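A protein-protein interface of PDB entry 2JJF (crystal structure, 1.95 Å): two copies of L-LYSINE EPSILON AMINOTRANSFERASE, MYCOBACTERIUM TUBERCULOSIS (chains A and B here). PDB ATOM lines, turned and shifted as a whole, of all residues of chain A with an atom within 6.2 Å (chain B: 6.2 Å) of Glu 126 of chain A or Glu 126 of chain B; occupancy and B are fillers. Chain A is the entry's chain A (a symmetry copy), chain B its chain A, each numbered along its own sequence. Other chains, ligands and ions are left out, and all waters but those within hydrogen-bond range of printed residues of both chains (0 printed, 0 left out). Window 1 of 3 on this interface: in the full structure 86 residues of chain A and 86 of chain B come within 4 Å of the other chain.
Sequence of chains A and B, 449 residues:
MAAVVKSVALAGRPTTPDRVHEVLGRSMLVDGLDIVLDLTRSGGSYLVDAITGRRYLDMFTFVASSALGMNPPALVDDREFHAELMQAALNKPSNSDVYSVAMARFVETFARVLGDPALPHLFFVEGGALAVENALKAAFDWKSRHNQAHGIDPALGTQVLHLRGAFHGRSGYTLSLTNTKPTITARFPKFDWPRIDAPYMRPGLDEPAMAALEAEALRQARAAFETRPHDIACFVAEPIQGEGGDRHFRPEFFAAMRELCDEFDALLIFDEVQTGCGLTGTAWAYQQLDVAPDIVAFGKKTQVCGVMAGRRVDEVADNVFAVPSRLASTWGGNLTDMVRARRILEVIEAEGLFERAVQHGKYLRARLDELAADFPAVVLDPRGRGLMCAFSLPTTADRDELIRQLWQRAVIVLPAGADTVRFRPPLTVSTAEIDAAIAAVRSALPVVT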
ATOM      1  N   LYS A  92     -32.127  28.026  -8.069  1.00  0.00           N
ATOM      2  CA  LYS A  92     -31.359  27.304  -7.062  1.00  0.00           C
ATOM      3  C   LYS A  92     -31.887  25.877  -7.012  1.00  0.00           C
ATOM      4  O   LYS A  92     -32.748  25.558  -6.189  1.00  0.00           O
ATOM      5  CB  LYS A  92     -31.440  27.986  -5.688  1.00  0.00           C
ATOM      6  CG  LYS A  92     -30.462  27.404  -4.659  1.00  0.00           C
ATOM      7  CD  LYS A  92     -30.526  28.118  -3.305  1.00  0.00           C
ATOM      8  CE  LYS A  92     -29.405  27.599  -2.404  1.00  0.00           C
ATOM      9  NZ  LYS A  92     -29.359  28.285  -1.079  1.00  0.00           N
ATOM     10  N   PHE A 124     -21.175  17.251  -0.935  1.00  0.00           N
ATOM     11  CA  PHE A 124     -21.242  18.712  -0.861  1.00  0.00           C
ATOM     12  C   PHE A 124     -22.452  19.199  -0.084  1.00  0.00           C
ATOM     13  O   PHE A 124     -23.520  18.576  -0.090  1.00  0.00           O
ATOM     14  CB  PHE A 124     -21.212  19.331  -2.266  1.00  0.00           C
ATOM     15  CG  PHE A 124     -19.994  18.949  -3.051  1.00  0.00           C
ATOM     16  CD1 PHE A 124     -18.765  19.560  -2.790  1.00  0.00           C
ATOM     17  CD2 PHE A 124     -20.063  17.950  -4.021  1.00  0.00           C
ATOM     18  CE1 PHE A 124     -17.619  19.191  -3.503  1.00  0.00           C
ATOM     19  CE2 PHE A 124     -18.925  17.575  -4.743  1.00  0.00           C
ATOM     20  CZ  PHE A 124     -17.706  18.190  -4.482  1.00  0.00           C
ATOM     21  N   VAL A 125     -22.265  20.334   0.575  1.00  0.00           N
ATOM     22  CA  VAL A 125     -23.271  20.900   1.461  1.00  0.00           C
ATOM     23  C   VAL A 125     -22.984  22.413   1.590  1.00  0.00           C
ATOM     24  O   VAL A 125     -21.874  22.866   1.280  1.00  0.00           O
ATOM     25  CB  VAL A 125     -23.243  20.168   2.839  1.00  0.00           C
ATOM     26  CG1 VAL A 125     -21.954  20.499   3.625  1.00  0.00           C
ATOM     27  CG2 VAL A 125     -24.481  20.479   3.662  1.00  0.00           C
ATOM     28  N   GLU A 126     -23.978  23.186   2.018  1.00  0.00           N
ATOM     29  CA  GLU A 126     -23.755  24.599   2.340  1.00  0.00           C
ATOM     30  C   GLU A 126     -23.270  24.685   3.784  1.00  0.00           C
ATOM     31  O   GLU A 126     -23.931  24.163   4.682  1.00  0.00           O
ATOM     32  CB  GLU A 126     -25.053  25.409   2.213  1.00  0.00           C
ATOM     33  CG  GLU A 126     -25.594  25.578   0.793  1.00  0.00           C
ATOM     34  CD  GLU A 126     -26.813  26.520   0.731  1.00  0.00           C
ATOM     35  OE1 GLU A 126     -27.668  26.480   1.641  1.00  0.00           O
ATOM     36  OE2 GLU A 126     -26.915  27.296  -0.237  1.00  0.00           O
ATOM     37  N   GLY A 127     -22.127  25.336   4.002  1.00  0.00           N
ATOM     38  CA  GLY A 127     -21.663  25.661   5.356  1.00  0.00           C
ATOM     39  C   GLY A 127     -20.528  24.792   5.863  1.00  0.00           C
ATOM     40  O   GLY A 127     -20.573  23.560   5.735  1.00  0.00           O
ATOM     41  N   GLY A 128     -19.519  25.436   6.454  1.00  0.00           N
ATOM     42  CA  GLY A 128     -18.352  24.729   6.988  1.00  0.00           C
ATOM     43  C   GLY A 128     -18.648  23.837   8.192  1.00  0.00           C
ATOM     44  O   GLY A 128     -18.118  22.726   8.291  1.00  0.00           O
ATOM     45  N   LEU A 130     -21.445  22.310   8.875  1.00  0.00           N
ATOM     46  CA  LEU A 130     -22.140  21.136   8.345  1.00  0.00           C
ATOM     47  C   LEU A 130     -21.220  20.169   7.593  1.00  0.00           C
ATOM     48  O   LEU A 130     -21.450  18.960   7.615  1.00  0.00           O
ATOM     49  CB  LEU A 130     -23.324  21.553   7.477  1.00  0.00           C
ATOM     50  CG  LEU A 130     -24.708  21.196   8.029  1.00  0.00           C
ATOM     51  CD1 LEU A 130     -24.806  21.303   9.545  1.00  0.00           C
ATOM     52  CD2 LEU A 130     -25.768  22.040   7.354  1.00  0.00           C
ATOM     53  N   ALA A 131     -20.196  20.697   6.929  1.00  0.00           N
ATOM     54  CA  ALA A 131     -19.155  19.854   6.325  1.00  0.00           C
ATOM     55  C   ALA A 131     -18.486  19.004   7.410  1.00  0.00           C
ATOM     56  O   ALA A 131     -18.386  17.783   7.270  1.00  0.00           O
ATOM     57  CB  ALA A 131     -18.118  20.704   5.587  1.00  0.00           C
ATOM     58  N   GLN A 303     -15.997  27.716  -1.484  1.00  0.00           N
ATOM     59  CA  GLN A 303     -17.318  28.349  -1.708  1.00  0.00           C
ATOM     60  C   GLN A 303     -18.461  27.404  -1.351  1.00  0.00           C
ATOM     61  O   GLN A 303     -19.295  27.716  -0.491  1.00  0.00           O
ATOM     62  CB  GLN A 303     -17.460  28.912  -3.144  1.00  0.00           C
ATOM     63  CG  GLN A 303     -16.306  29.849  -3.547  1.00  0.00           C
ATOM     64  CD  GLN A 303     -16.373  31.190  -2.849  1.00  0.00           C
ATOM     65  OE1 GLN A 303     -17.058  32.096  -3.316  1.00  0.00           O
ATOM     66  NE2 GLN A 303     -15.663  31.329  -1.719  1.00  0.00           N
ATOM     67  N   VAL A 304     -18.495  26.261  -2.028  1.00  0.00           N
ATOM     68  CA  VAL A 304     -19.308  25.128  -1.597  1.00  0.00           C
ATOM     69  C   VAL A 304     -18.485  24.312  -0.586  1.00  0.00           C
ATOM     70  O   VAL A 304     -17.263  24.214  -0.699  1.00  0.00           O
ATOM     71  CB  VAL A 304     -19.816  24.275  -2.815  1.00  0.00           C
ATOM     72  CG1 VAL A 304     -18.664  23.675  -3.578  1.00  0.00           C
ATOM     73  CG2 VAL A 304     -20.804  23.186  -2.368  1.00  0.00           C
ATOM     74  N   CYS A 305     -19.147  23.778   0.426  1.00  0.00           N
ATOM     75  CA  CYS A 305     -18.450  23.058   1.488  1.00  0.00           C
ATOM     76  C   CYS A 305     -18.688  21.559   1.306  1.00  0.00           C
ATOM     77  O   CYS A 305     -19.498  21.153   0.470  1.00  0.00           O
ATOM     78  CB  CYS A 305     -18.929  23.549   2.850  1.00  0.00           C
ATOM     79  SG  CYS A 305     -18.720  25.347   3.010  1.00  0.00           S
ATOM     80  N   SER A 329     -28.961  17.012   2.304  1.00  0.00           N
ATOM     81  CA  SER A 329     -29.572  18.305   2.604  1.00  0.00           C
ATOM     82  C   SER A 329     -30.515  18.597   1.441  1.00  0.00           C
ATOM     83  O   SER A 329     -30.478  17.892   0.423  1.00  0.00           O
ATOM     84  CB  SER A 329     -28.502  19.400   2.759  1.00  0.00           C
ATOM     85  OG  SER A 329     -27.831  19.672   1.531  1.00  0.00           O
ATOM     86  N   TRP A 331     -30.510  21.239  -0.736  1.00  0.00           N
ATOM     87  CA  TRP A 331     -29.883  21.764  -1.958  1.00  0.00           C
ATOM     88  C   TRP A 331     -28.651  21.013  -2.471  1.00  0.00           C
ATOM     89  O   TRP A 331     -28.361  21.066  -3.670  1.00  0.00           O
ATOM     90  CB  TRP A 331     -29.573  23.257  -1.817  1.00  0.00           C
ATOM     91  CG  TRP A 331     -30.806  24.123  -1.885  1.00  0.00           C
ATOM     92  CD1 TRP A 331     -31.704  24.197  -2.915  1.00  0.00           C
ATOM     93  CD2 TRP A 331     -31.259  25.057  -0.886  1.00  0.00           C
ATOM     94  NE1 TRP A 331     -32.693  25.114  -2.618  1.00  0.00           N
ATOM     95  CE2 TRP A 331     -32.442  25.656  -1.381  1.00  0.00           C
ATOM     96  CE3 TRP A 331     -30.777  25.443   0.374  1.00  0.00           C
ATOM     97  CZ2 TRP A 331     -33.155  26.626  -0.657  1.00  0.00           C
ATOM     98  CZ3 TRP A 331     -31.487  26.407   1.099  1.00  0.00           C
ATOM     99  CH2 TRP A 331     -32.661  26.985   0.580  1.00  0.00           C
ATOM    100  N   GLY A 332     -27.939  20.330  -1.571  1.00  0.00           N
ATOM    101  CA  GLY A 332     -26.672  19.653  -1.912  1.00  0.00           C
ATOM    102  C   GLY A 332     -25.606  20.659  -2.342  1.00  0.00           C
ATOM    103  O   GLY A 332     -24.882  20.445  -3.319  1.00  0.00           O
ATOM    104  N   GLY A 333     -25.528  21.767  -1.616  1.00  0.00           N
ATOM    105  CA  GLY A 333     -24.622  22.853  -1.983  1.00  0.00           C
ATOM    106  C   GLY A 333     -25.320  23.829  -2.917  1.00  0.00           C
ATOM    107  O   GLY A 333     -26.346  23.504  -3.527  1.00  0.00           O
ATOM    108  N   ASN A 334     -24.767  25.029  -3.017  1.00  0.00           N
ATOM    109  CA  ASN A 334     -25.330  26.078  -3.840  1.00  0.00           C
ATOM    110  C   ASN A 334     -24.741  25.996  -5.255  1.00  0.00           C
ATOM    111  O   ASN A 334     -23.523  26.083  -5.426  1.00  0.00           O
ATOM    112  CB  ASN A 334     -25.024  27.441  -3.195  1.00  0.00           C
ATOM    113  CG  ASN A 334     -25.867  28.561  -3.759  1.00  0.00           C
ATOM    114  OD1 ASN A 334     -25.962  28.725  -4.973  1.00  0.00           O
ATOM    115  ND2 ASN A 334     -26.487  29.347  -2.873  1.00  0.00           N
ATOM    116  N   ASP A 337     -22.370  28.760  -6.215  1.00  0.00           N
ATOM    117  CA  ASP A 337     -21.051  28.566  -5.608  1.00  0.00           C
ATOM    118  C   ASP A 337     -20.211  27.525  -6.357  1.00  0.00           C
ATOM    119  O   ASP A 337     -19.002  27.695  -6.493  1.00  0.00           O
ATOM    120  CB  ASP A 337     -21.183  28.164  -4.134  1.00  0.00           C
ATOM    121  CG  ASP A 337     -21.682  29.305  -3.257  1.00  0.00           C
ATOM    122  OD1 ASP A 337     -21.591  30.489  -3.654  1.00  0.00           O
ATOM    123  OD2 ASP A 337     -22.158  29.009  -2.161  1.00  0.00           O
ATOM    124  N   LYS B  92     -18.403  36.311  -2.909  1.00  0.00           N
ATOM    125  CA  LYS B  92     -19.215  35.797  -1.813  1.00  0.00           C
ATOM    126  C   LYS B  92     -18.715  36.438  -0.526  1.00  0.00           C
ATOM    127  O   LYS B  92     -17.887  35.858   0.179  1.00  0.00           O
ATOM    128  CB  LYS B  92     -19.165  34.263  -1.739  1.00  0.00           C
ATOM    129  CG  LYS B  92     -20.186  33.666  -0.761  1.00  0.00           C
ATOM    130  CD  LYS B  92     -20.150  32.134  -0.724  1.00  0.00           C
ATOM    131  CE  LYS B  92     -21.309  31.621   0.132  1.00  0.00           C
ATOM    132  NZ  LYS B  92     -21.384  30.131   0.175  1.00  0.00           N
ATOM    133  N   PHE B 124     -29.771  35.527   9.624  1.00  0.00           N
ATOM    134  CA  PHE B 124     -29.680  34.750   8.386  1.00  0.00           C
ATOM    135  C   PHE B 124     -28.486  33.812   8.376  1.00  0.00           C
ATOM    136  O   PHE B 124     -27.430  34.101   8.951  1.00  0.00           O
ATOM    137  CB  PHE B 124     -29.654  35.676   7.162  1.00  0.00           C
ATOM    138  CG  PHE B 124     -30.853  36.570   7.076  1.00  0.00           C
ATOM    139  CD1 PHE B 124     -32.078  36.068   6.630  1.00  0.00           C
ATOM    140  CD2 PHE B 124     -30.772  37.902   7.479  1.00  0.00           C
ATOM    141  CE1 PHE B 124     -33.208  36.891   6.570  1.00  0.00           C
ATOM    142  CE2 PHE B 124     -31.894  38.737   7.419  1.00  0.00           C
ATOM    143  CZ  PHE B 124     -33.110  38.232   6.971  1.00  0.00           C
ATOM    144  N   VAL B 125     -28.673  32.688   7.700  1.00  0.00           N
ATOM    145  CA  VAL B 125     -27.685  31.620   7.668  1.00  0.00           C
ATOM    146  C   VAL B 125     -27.948  30.776   6.400  1.00  0.00           C
ATOM    147  O   VAL B 125     -29.039  30.847   5.818  1.00  0.00           O
ATOM    148  CB  VAL B 125     -27.770  30.773   8.975  1.00  0.00           C
ATOM    149  CG1 VAL B 125     -29.076  29.949   9.028  1.00  0.00           C
ATOM    150  CG2 VAL B 125     -26.553  29.880   9.143  1.00  0.00           C
ATOM    151  N   GLU B 126     -26.953  30.008   5.964  1.00  0.00           N
ATOM    152  CA  GLU B 126     -27.160  29.042   4.879  1.00  0.00           C
ATOM    153  C   GLU B 126     -27.689  27.749   5.491  1.00  0.00           C
ATOM    154  O   GLU B 126     -27.067  27.206   6.404  1.00  0.00           O
ATOM    155  CB  GLU B 126     -25.844  28.735   4.152  1.00  0.00           C
ATOM    156  CG  GLU B 126     -25.256  29.883   3.331  1.00  0.00           C
ATOM    157  CD  GLU B 126     -24.018  29.456   2.516  1.00  0.00           C
ATOM    158  OE1 GLU B 126     -23.193  28.665   3.020  1.00  0.00           O
ATOM    159  OE2 GLU B 126     -23.872  29.922   1.371  1.00  0.00           O
ATOM    160  N   GLY B 127     -28.826  27.263   4.992  1.00  0.00           N
ATOM    161  CA  GLY B 127     -29.326  25.931   5.352  1.00  0.00           C
ATOM    162  C   GLY B 127     -30.493  25.931   6.322  1.00  0.00           C
ATOM    163  O   GLY B 127     -30.466  26.642   7.337  1.00  0.00           O
ATOM    164  N   GLY B 128     -31.507  25.121   6.015  1.00  0.00           N
ATOM    165  CA  GLY B 128     -32.704  25.019   6.855  1.00  0.00           C
ATOM    166  C   GLY B 128     -32.463  24.397   8.229  1.00  0.00           C
ATOM    167  O   GLY B 128     -33.016  24.861   9.230  1.00  0.00           O
ATOM    168  N   LEU B 130     -29.717  24.492   9.982  1.00  0.00           N
ATOM    169  CA  LEU B 130     -29.028  25.513  10.772  1.00  0.00           C
ATOM    170  C   LEU B 130     -29.941  26.657  11.222  1.00  0.00           C
ATOM    171  O   LEU B 130     -29.734  27.223  12.295  1.00  0.00           O
ATOM    172  CB  LEU B 130     -27.809  26.047  10.023  1.00  0.00           C
ATOM    173  CG  LEU B 130     -26.450  25.713  10.647  1.00  0.00           C
ATOM    174  CD1 LEU B 130     -26.398  24.335  11.293  1.00  0.00           C
ATOM    175  CD2 LEU B 130     -25.354  25.872   9.615  1.00  0.00           C
ATOM    176  N   ALA B 131     -30.934  26.999  10.405  1.00  0.00           N
ATOM    177  CA  ALA B 131     -31.971  27.956  10.816  1.00  0.00           C
ATOM    178  C   ALA B 131     -32.689  27.436  12.064  1.00  0.00           C
ATOM    179  O   ALA B 131     -32.807  28.153  13.059  1.00  0.00           O
ATOM    180  CB  ALA B 131     -32.968  28.207   9.682  1.00  0.00           C
ATOM    181  N   GLN B 303     -34.735  31.009   0.054  1.00  0.00           N
ATOM    182  CA  GLN B 303     -33.396  30.872  -0.566  1.00  0.00           C
ATOM    183  C   GLN B 303     -32.282  30.999   0.468  1.00  0.00           C
ATOM    184  O   GLN B 303     -31.471  30.080   0.641  1.00  0.00           O
ATOM    185  CB  GLN B 303     -33.198  31.849  -1.751  1.00  0.00           C
ATOM    186  CG  GLN B 303     -34.322  31.767  -2.802  1.00  0.00           C
ATOM    187  CD  GLN B 303     -34.252  30.503  -3.632  1.00  0.00           C
ATOM    188  OE1 GLN B 303     -33.536  30.458  -4.628  1.00  0.00           O
ATOM    189  NE2 GLN B 303     -34.995  29.462  -3.226  1.00  0.00           N
ATOM    190  N   VAL B 304     -32.248  32.146   1.140  1.00  0.00           N
ATOM    191  CA  VAL B 304     -31.471  32.306   2.364  1.00  0.00           C
ATOM    192  C   VAL B 304     -32.340  31.835   3.542  1.00  0.00           C
ATOM    193  O   VAL B 304     -33.559  32.004   3.535  1.00  0.00           O
ATOM    194  CB  VAL B 304     -30.940  33.775   2.533  1.00  0.00           C
ATOM    195  CG1 VAL B 304     -32.079  34.755   2.649  1.00  0.00           C
ATOM    196  CG2 VAL B 304     -29.988  33.897   3.732  1.00  0.00           C
ATOM    197  N   CYS B 305     -31.720  31.199   4.521  1.00  0.00           N
ATOM    198  CA  CYS B 305     -32.463  30.635   5.644  1.00  0.00           C
ATOM    199  C   CYS B 305     -32.248  31.519   6.872  1.00  0.00           C
ATOM    200  O   CYS B 305     -31.419  32.432   6.846  1.00  0.00           O
ATOM    201  CB  CYS B 305     -32.019  29.198   5.892  1.00  0.00           C
ATOM    202  SG  CYS B 305     -32.199  28.187   4.393  1.00  0.00           S
ATOM    203  N   SER B 329     -22.098  32.670  11.652  1.00  0.00           N
ATOM    204  CA  SER B 329     -21.472  31.768  10.688  1.00  0.00           C
ATOM    205  C   SER B 329     -20.488  32.624   9.897  1.00  0.00           C
ATOM    206  O   SER B 329     -20.506  33.857  10.017  1.00  0.00           O
ATOM    207  CB  SER B 329     -22.526  31.119   9.773  1.00  0.00           C
ATOM    208  OG  SER B 329     -23.153  32.071   8.918  1.00  0.00           O
ATOM    209  N   TRP B 331     -20.375  33.239   6.532  1.00  0.00           N
ATOM    210  CA  TRP B 331     -20.954  34.063   5.459  1.00  0.00           C
ATOM    211  C   TRP B 331     -22.183  34.899   5.827  1.00  0.00           C
ATOM    212  O   TRP B 331     -22.433  35.926   5.189  1.00  0.00           O
ATOM    213  CB  TRP B 331     -21.240  33.219   4.215  1.00  0.00           C
ATOM    214  CG  TRP B 331     -19.990  32.834   3.464  1.00  0.00           C
ATOM    215  CD1 TRP B 331     -19.058  33.680   2.927  1.00  0.00           C
ATOM    216  CD2 TRP B 331     -19.551  31.498   3.148  1.00  0.00           C
ATOM    217  NE1 TRP B 331     -18.063  32.957   2.301  1.00  0.00           N
ATOM    218  CE2 TRP B 331     -18.343  31.617   2.421  1.00  0.00           C
ATOM    219  CE3 TRP B 331     -20.066  30.218   3.408  1.00  0.00           C
ATOM    220  CZ2 TRP B 331     -17.635  30.499   1.948  1.00  0.00           C
ATOM    221  CZ3 TRP B 331     -19.361  29.103   2.940  1.00  0.00           C
ATOM    222  CH2 TRP B 331     -18.160  29.254   2.220  1.00  0.00           C
ATOM    223  N   GLY B 332     -22.935  34.458   6.839  1.00  0.00           N
ATOM    224  CA  GLY B 332     -24.203  35.109   7.224  1.00  0.00           C
ATOM    225  C   GLY B 332     -25.236  35.015   6.103  1.00  0.00           C
ATOM    226  O   GLY B 332     -25.933  35.985   5.792  1.00  0.00           O
ATOM    227  N   GLY B 333     -25.317  33.843   5.486  1.00  0.00           N
ATOM    228  CA  GLY B 333     -26.190  33.652   4.331  1.00  0.00           C
ATOM    229  C   GLY B 333     -25.445  33.980   3.046  1.00  0.00           C
ATOM    230  O   GLY B 333     -24.406  34.651   3.066  1.00  0.00           O
ATOM    231  N   ASN B 334     -25.972  33.493   1.932  1.00  0.00           N
ATOM    232  CA  ASN B 334     -25.364  33.691   0.633  1.00  0.00           C
ATOM    233  C   ASN B 334     -25.910  34.978  -0.001  1.00  0.00           C
ATOM    234  O   ASN B 334     -27.120  35.107  -0.198  1.00  0.00           O
ATOM    235  CB  ASN B 334     -25.666  32.470  -0.253  1.00  0.00           C
ATOM    236  CG  ASN B 334     -24.785  32.402  -1.478  1.00  0.00           C
ATOM    237  OD1 ASN B 334     -24.648  33.381  -2.209  1.00  0.00           O
ATOM    238  ND2 ASN B 334     -24.178  31.234  -1.715  1.00  0.00           N
ATOM    239  N   ASP B 337     -28.198  34.515  -2.956  1.00  0.00           N
ATOM    240  CA  ASP B 337     -29.538  34.103  -2.533  1.00  0.00           C
ATOM    241  C   ASP B 337     -30.374  35.279  -2.015  1.00  0.00           C
ATOM    242  O   ASP B 337     -31.574  35.338  -2.267  1.00  0.00           O
ATOM    243  CB  ASP B 337     -29.461  33.009  -1.462  1.00  0.00           C
ATOM    244  CG  ASP B 337     -28.968  31.679  -2.017  1.00  0.00           C
ATOM    245  OD1 ASP B 337     -29.025  31.451  -3.246  1.00  0.00           O
ATOM    246  OD2 ASP B 337     -28.533  30.857  -1.210  1.00  0.00           O
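The backbone NH (N) of Val 125 of chain B is in hydrogen-bond range of the backbone carbonyl oxygen (O) of Cys 305 of chain B, 2.9 Å away.
The side-chain carboxylate (OE2) of Glu 126 of chain A sits at hydrogen-bond distance from the side-chain amide nitrogen (ND2) of Asn 334 of chain A, at 3.4 Å.
SG of Cys 305 of chain B sits at hydrogen-bond distance from N of Gly 128 of chain B, at 3.5 Å.
The side-chain carboxylate (OE2) of Glu 126 of chain B is in hydrogen-bond range of the side-chain amide nitrogen (ND2) of Asn 334 of chain B (3.4 Å).
The side-chain sulfur (SG) of Cys 305 of chain A lies close to the backbone NH (N) of Gly 127 of chain A, at 3.5 Å.
O of Cys 305 of chain A lies within hydrogen-bond range of N of Val 125 of chain A (2.9 Å).
Of chain B, only Glu 126 and Gly 127 come within 4 Å of Glu 126 of chain A.
Glu 126 of chain B touches just these residues of chain A: Glu 126 (3.8 Å) and Gly 127 (3.6 Å).
Of the printed residues of chain B, Cys 305 of chain A touches Trp 331.
Of the printed residues of chain A, Asn 334 of chain B touches Asn 334 (3.2 Å) and Asp 337 (3.0 Å).
Gly 333 of chain B touches none of the printed residues of chain A.
The nearest residue of chain B that does not touch Glu 126 of chain A is Asp 337 of chain B (4.03 Å).
The nearest residue of chain A that does not touch Glu 126 of chain B is Asp 337 of chain A (4.03 Å).
OD2 of Asp 337 of chain A is in salt-bridge range of NZ of Lys 92 of chain B, at 2.7 Å.
The side-chain amino group of Lys 92 of chain B lies within hydrogen-bond range of the backbone carbonyl oxygen of Gln 303 of chain A.
The side-chain carboxylate of Asp 337 of chain B lies within salt-bridge range of the side-chain amino group of Lys 92 of chain A.
ND2 of Asn 334 of chain B is in hydrogen-bond range of OD2 of Asp 337 of chain A, at 3.0 Å.
ND2 of Asn 334 of chain B lies close to ND2 of Asn 334 of chain A (3.2 Å).
The backbone carbonyl oxygen (O) of Gln 303 of chain B sits at hydrogen-bond distance from the side-chain amino group (NZ) of Lys 92 of chain A (3.3 Å).
OD2 of Asp 337 of chain B lies within hydrogen-bond range of ND2 of Asn 334 of chain A, 3.0 Å away.
Glu 126 of chain A touches Gly 127 of chain B, and with the chains exchanged Gly 127 of chain A touches Glu 126 of chain B.
Gln 303 of chain A touches Trp 331 of chain B, and with the chains exchanged Trp 331 of chain A touches Gln 303 of chain B.
Cys 305 of chain A touches Trp 331 of chain B, and with the chains exchanged Trp 331 of chain A touches Cys 305 of chain B.
Asn 334 of chain B touches its own counterpart, Asn 334 of chain A.
Positions printed for both chains: 92, 124, 125, 126, 127, 128, 130, 131, 303, 304, 305, 329, 331, 332, 333, 334 and 337.
Of the 15 pairs that touch across the chains among the printed residues, 15 have their exchanged pair printed and touching as well.
Of the 17 printed residues of chain B, 9 touch a printed residue of chain A.
Hydrophobic or aromatic side chains of chain B within 4 Å of the printed part of chain A: Leu 130 and Trp 331.
Among the printed residues, 15 pairs touch across the chains.
Among the printed residues, pairs that only touch across the chains: Trp 331 of chain A with Gln 303 of chain B, Gln 303 of chain A with Trp 331 of chain B, Gly 127 of chain A with Glu 126 of chain B, Glu 126 of chain A with Gly 127 of chain B, Cys 305 of chain A with Trp 331 of chain B, Trp 331 of chain A with Cys 305 of chain B, Glu 126 of chain A with Glu 126 of chain B and Leu 130 of chain A with Leu 130 of chain B.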
